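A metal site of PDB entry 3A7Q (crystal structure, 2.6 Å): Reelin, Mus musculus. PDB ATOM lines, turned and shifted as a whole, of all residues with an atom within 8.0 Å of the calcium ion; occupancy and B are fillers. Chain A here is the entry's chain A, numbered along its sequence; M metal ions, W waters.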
ATOM      1  N   ASP A 227     -21.708 -14.100   4.984  1.00  0.00           N
ATOM      2  CA  ASP A 227     -21.609 -13.515   3.650  1.00  0.00           C
ATOM      3  C   ASP A 227     -21.634 -11.985   3.595  1.00  0.00           C
ATOM      4  O   ASP A 227     -22.637 -11.340   3.947  1.00  0.00           O
ATOM      5  CB  ASP A 227     -22.642 -14.104   2.678  1.00  0.00           C
ATOM      6  CG  ASP A 227     -22.083 -14.271   1.265  1.00  0.00           C
ATOM      7  OD1 ASP A 227     -22.274 -15.359   0.687  1.00  0.00           O
ATOM      8  OD2 ASP A 227     -21.435 -13.335   0.727  1.00  0.00           O
ATOM      9  N   ASP A 228     -20.496 -11.457   3.142  1.00  0.00           N
ATOM     10  CA  ASP A 228     -20.209 -10.027   2.953  1.00  0.00           C
ATOM     11  C   ASP A 228     -20.579  -9.547   1.551  1.00  0.00           C
ATOM     12  O   ASP A 228     -20.671  -8.344   1.300  1.00  0.00           O
ATOM     13  CB  ASP A 228     -18.701  -9.769   3.173  1.00  0.00           C
ATOM     14  CG  ASP A 228     -17.819 -10.807   2.451  1.00  0.00           C
ATOM     15  OD1 ASP A 228     -16.777 -10.411   1.893  1.00  0.00           O
ATOM     16  OD2 ASP A 228     -18.142 -12.012   2.445  1.00  0.00           O
ATOM     17  N   PHE A 229     -20.756 -10.521   0.647  1.00  0.00           N
ATOM     18  CA  PHE A 229     -20.966 -10.304  -0.793  1.00  0.00           C
ATOM     19  C   PHE A 229     -19.828  -9.547  -1.501  1.00  0.00           C
ATOM     20  O   PHE A 229     -19.970  -9.146  -2.661  1.00  0.00           O
ATOM     21  CB  PHE A 229     -22.326  -9.666  -1.075  1.00  0.00           C
ATOM     22  CG  PHE A 229     -23.465 -10.373  -0.417  1.00  0.00           C
ATOM     23  CD1 PHE A 229     -23.828 -11.659  -0.822  1.00  0.00           C
ATOM     24  CD2 PHE A 229     -24.158  -9.780   0.617  1.00  0.00           C
ATOM     25  CE1 PHE A 229     -24.871 -12.332  -0.185  1.00  0.00           C
ATOM     26  CE2 PHE A 229     -25.202 -10.453   1.254  1.00  0.00           C
ATOM     27  CZ  PHE A 229     -25.563 -11.725   0.849  1.00  0.00           C
ATOM     28  N   GLU A 230     -18.694  -9.392  -0.819  1.00  0.00           N
ATOM     29  CA  GLU A 230     -17.517  -8.767  -1.411  1.00  0.00           C
ATOM     30  C   GLU A 230     -16.741  -9.766  -2.296  1.00  0.00           C
ATOM     31  O   GLU A 230     -15.728  -9.402  -2.906  1.00  0.00           O
ATOM     32  CB  GLU A 230     -16.601  -8.160  -0.341  1.00  0.00           C
ATOM     33  CG  GLU A 230     -17.277  -7.257   0.722  1.00  0.00           C
ATOM     34  CD  GLU A 230     -18.107  -6.113   0.150  1.00  0.00           C
ATOM     35  OE1 GLU A 230     -17.813  -5.659  -0.986  1.00  0.00           O
ATOM     36  OE2 GLU A 230     -19.049  -5.652   0.826  1.00  0.00           O
ATOM     37  N   GLY A 231     -17.252 -10.996  -2.385  1.00  0.00           N
ATOM     38  CA  GLY A 231     -16.576 -12.078  -3.100  1.00  0.00           C
ATOM     39  C   GLY A 231     -16.948 -12.223  -4.572  1.00  0.00           C
ATOM     40  O   GLY A 231     -16.082 -12.434  -5.425  1.00  0.00           O
ATOM     41  N   SER A 247     -24.468  -5.522  -5.909  1.00  0.00           N
ATOM     42  CA  SER A 247     -24.429  -4.132  -6.349  1.00  0.00           C
ATOM     43  C   SER A 247     -23.848  -3.231  -5.269  1.00  0.00           C
ATOM     44  O   SER A 247     -23.765  -3.627  -4.113  1.00  0.00           O
ATOM     45  CB  SER A 247     -25.841  -3.652  -6.671  1.00  0.00           C
ATOM     46  OG  SER A 247     -26.470  -4.528  -7.606  1.00  0.00           O
ATOM     47  N   ILE A 252     -25.774   0.296   2.497  1.00  0.00           N
ATOM     48  CA  ILE A 252     -25.583   0.621   3.906  1.00  0.00           C
ATOM     49  C   ILE A 252     -24.073   0.793   4.140  1.00  0.00           C
ATOM     50  O   ILE A 252     -23.604   1.906   4.376  1.00  0.00           O
ATOM     51  CB  ILE A 252     -26.182  -0.450   4.859  1.00  0.00           C
ATOM     52  CG1 ILE A 252     -27.635  -0.768   4.487  1.00  0.00           C
ATOM     53  CG2 ILE A 252     -26.092   0.012   6.317  1.00  0.00           C
ATOM     54  CD1 ILE A 252     -27.824  -2.162   3.904  1.00  0.00           C
ATOM     55  N   LEU A 253     -23.333  -0.312   4.039  1.00  0.00           N
ATOM     56  CA  LEU A 253     -21.905  -0.388   4.396  1.00  0.00           C
ATOM     57  C   LEU A 253     -20.941   0.038   3.286  1.00  0.00           C
ATOM     58  O   LEU A 253     -20.746  -0.679   2.302  1.00  0.00           O
ATOM     59  CB  LEU A 253     -21.557  -1.793   4.885  1.00  0.00           C
ATOM     60  CG  LEU A 253     -21.863  -2.140   6.339  1.00  0.00           C
ATOM     61  CD1 LEU A 253     -22.457  -3.505   6.399  1.00  0.00           C
ATOM     62  CD2 LEU A 253     -20.619  -2.031   7.249  1.00  0.00           C
ATOM     63  N   SER A 254     -20.295   1.192   3.492  1.00  0.00           N
ATOM     64  CA  SER A 254     -19.478   1.816   2.442  1.00  0.00           C
ATOM     65  C   SER A 254     -18.103   1.165   2.215  1.00  0.00           C
ATOM     66  O   SER A 254     -17.208   1.780   1.625  1.00  0.00           O
ATOM     67  CB  SER A 254     -19.336   3.329   2.697  1.00  0.00           C
ATOM     68  OG  SER A 254     -20.565   3.998   2.452  1.00  0.00           O
ATOM     69  N   SER A 255     -17.949  -0.073   2.683  1.00  0.00           N
ATOM     70  CA  SER A 255     -16.783  -0.903   2.343  1.00  0.00           C
ATOM     71  C   SER A 255     -16.952  -1.514   0.950  1.00  0.00           C
ATOM     72  O   SER A 255     -16.024  -1.469   0.136  1.00  0.00           O
ATOM     73  CB  SER A 255     -16.558  -2.022   3.382  1.00  0.00           C
ATOM     74  OG  SER A 255     -15.686  -1.595   4.421  1.00  0.00           O
ATOM     75  N   GLY A 256     -18.143  -2.071   0.683  1.00  0.00           N
ATOM     76  CA  GLY A 256     -18.431  -2.607  -0.641  1.00  0.00           C
ATOM     77  C   GLY A 256     -19.824  -3.123  -0.972  1.00  0.00           C
ATOM     78  O   GLY A 256     -20.841  -2.519  -0.606  1.00  0.00           O
ATOM     79  N   ASN A 257     -19.848  -4.247  -1.672  1.00  0.00           N
ATOM     80  CA  ASN A 257     -21.027  -4.775  -2.350  1.00  0.00           C
ATOM     81  C   ASN A 257     -22.143  -5.243  -1.421  1.00  0.00           C
ATOM     82  O   ASN A 257     -21.891  -5.683  -0.296  1.00  0.00           O
ATOM     83  CB  ASN A 257     -20.630  -5.901  -3.311  1.00  0.00           C
ATOM     84  CG  ASN A 257     -19.729  -5.412  -4.440  1.00  0.00           C
ATOM     85  OD1 ASN A 257     -18.536  -5.686  -4.447  1.00  0.00           O
ATOM     86  ND2 ASN A 257     -20.308  -4.666  -5.383  1.00  0.00           N
ATOM     87  N   ASN A 258     -23.368  -5.150  -1.912  1.00  0.00           N
ATOM     88  CA  ASN A 258     -24.516  -5.714  -1.226  1.00  0.00           C
ATOM     89  C   ASN A 258     -25.354  -6.499  -2.219  1.00  0.00           C
ATOM     90  O   ASN A 258     -25.076  -6.484  -3.426  1.00  0.00           O
ATOM     91  CB  ASN A 258     -25.331  -4.626  -0.528  1.00  0.00           C
ATOM     92  CG  ASN A 258     -25.902  -3.596  -1.486  1.00  0.00           C
ATOM     93  OD1 ASN A 258     -26.453  -3.932  -2.538  1.00  0.00           O
ATOM     94  ND2 ASN A 258     -25.791  -2.330  -1.113  1.00  0.00           N
ATOM     95  N   LEU A 259     -26.379  -7.187  -1.723  1.00  0.00           N
ATOM     96  CA  LEU A 259     -27.292  -7.930  -2.601  1.00  0.00           C
ATOM     97  C   LEU A 259     -28.535  -7.097  -2.868  1.00  0.00           C
ATOM     98  O   LEU A 259     -29.308  -6.809  -1.953  1.00  0.00           O
ATOM     99  CB  LEU A 259     -27.643  -9.271  -1.963  1.00  0.00           C
ATOM    100  CG  LEU A 259     -27.817 -10.515  -2.837  1.00  0.00           C
ATOM    101  CD1 LEU A 259     -26.509 -10.939  -3.516  1.00  0.00           C
ATOM    102  CD2 LEU A 259     -28.315 -11.616  -1.941  1.00  0.00           C
ATOM    103  N   PHE A 285     -27.675  -6.848   7.598  1.00  0.00           N
ATOM    104  CA  PHE A 285     -28.101  -5.494   7.288  1.00  0.00           C
ATOM    105  C   PHE A 285     -29.222  -5.564   6.252  1.00  0.00           C
ATOM    106  O   PHE A 285     -29.194  -6.394   5.342  1.00  0.00           O
ATOM    107  CB  PHE A 285     -26.939  -4.634   6.787  1.00  0.00           C
ATOM    108  CG  PHE A 285     -25.943  -4.254   7.870  1.00  0.00           C
ATOM    109  CD1 PHE A 285     -26.013  -3.015   8.486  1.00  0.00           C
ATOM    110  CD2 PHE A 285     -24.946  -5.143   8.255  1.00  0.00           C
ATOM    111  CE1 PHE A 285     -25.095  -2.663   9.485  1.00  0.00           C
ATOM    112  CE2 PHE A 285     -24.029  -4.806   9.255  1.00  0.00           C
ATOM    113  CZ  PHE A 285     -24.098  -3.559   9.863  1.00  0.00           C
ATOM    114  N   ILE A 364     -29.874  -6.222   1.104  1.00  0.00           N
ATOM    115  CA  ILE A 364     -29.445  -7.040   2.221  1.00  0.00           C
ATOM    116  C   ILE A 364     -27.918  -7.238   2.159  1.00  0.00           C
ATOM    117  O   ILE A 364     -27.356  -7.427   1.079  1.00  0.00           O
ATOM    118  CB  ILE A 364     -30.231  -8.395   2.303  1.00  0.00           C
ATOM    119  CG1 ILE A 364     -29.969  -9.092   3.656  1.00  0.00           C
ATOM    120  CG2 ILE A 364     -29.937  -9.298   1.093  1.00  0.00           C
ATOM    121  CD1 ILE A 364     -30.670 -10.427   3.844  1.00  0.00           C
ATOM    122  N   ASP A 365     -27.270  -7.167   3.332  1.00  0.00           N
ATOM    123  CA  ASP A 365     -25.806  -7.253   3.443  1.00  0.00           C
ATOM    124  C   ASP A 365     -25.342  -7.841   4.782  1.00  0.00           C
ATOM    125  O   ASP A 365     -26.109  -7.888   5.748  1.00  0.00           O
ATOM    126  CB  ASP A 365     -25.189  -5.854   3.235  1.00  0.00           C
ATOM    127  CG  ASP A 365     -23.714  -5.896   2.836  1.00  0.00           C
ATOM    128  OD1 ASP A 365     -23.146  -6.999   2.610  1.00  0.00           O
ATOM    129  OD2 ASP A 365     -23.113  -4.808   2.741  1.00  0.00           O
ATOM    130  N   GLN A 366     -24.097  -8.276   4.835  1.00  0.00           N
ATOM    131  CA  GLN A 366     -23.469  -8.822   6.058  1.00  0.00           C
ATOM    132  C   GLN A 366     -24.376  -9.785   6.797  1.00  0.00           C
ATOM    133  O   GLN A 366     -24.862  -9.510   7.904  1.00  0.00           O
ATOM    134  CB  GLN A 366     -23.000  -7.704   7.010  1.00  0.00           C
ATOM    135  CG  GLN A 366     -21.797  -6.905   6.554  1.00  0.00           C
ATOM    136  CD  GLN A 366     -20.460  -7.646   6.615  1.00  0.00           C
ATOM    137  OE1 GLN A 366     -20.383  -8.819   6.978  1.00  0.00           O
ATOM    138  NE2 GLN A 366     -19.383  -6.935   6.264  1.00  0.00           N
ATOM    139  N   ILE A 367     -24.599 -10.933   6.168  1.00  0.00           N
ATOM    140  CA  ILE A 367     -25.392 -11.977   6.759  1.00  0.00           C
ATOM    141  C   ILE A 367     -24.488 -12.888   7.577  1.00  0.00           C
ATOM    142  O   ILE A 367     -23.498 -13.446   7.082  1.00  0.00           O
ATOM    143  CB  ILE A 367     -26.135 -12.764   5.695  1.00  0.00           C
ATOM    144  CG1 ILE A 367     -27.206 -11.881   5.064  1.00  0.00           C
ATOM    145  CG2 ILE A 367     -26.766 -14.021   6.285  1.00  0.00           C
ATOM    146  CD1 ILE A 367     -27.507 -12.203   3.640  1.00  0.00           C
HETATM  147 CA    CA M   1     -21.225  -5.902   1.942  1.00  0.00          CA
HETATM  148  O   HOH W   1     -21.001  -3.757   1.874  1.00  0.00           O
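Four residues have an atom within 4 Å of the calcium ion: Asp 228, Glu 230, Asn 257 and Asp 365. The nearest printed residue that does not touch the calcium ion is Gly 256 (4.3 Å).
The calcium ion is bound by water W1 (2.2 Å), the side-chain carboxylate (OD1) of Asp 365 (2.3 Å), the side-chain carboxylate (OD2) of Asp 365 (2.3 Å), the backbone carbonyl oxygen (O) of Asn 257 (2.3 Å), the side-chain carboxylate (OE2) of Glu 230 (2.5 Å) and the backbone carbonyl oxygen (O) of Asp 228 (2.6 Å).
O of Asp 365 sits at hydrogen-bond distance from N of Phe 285.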
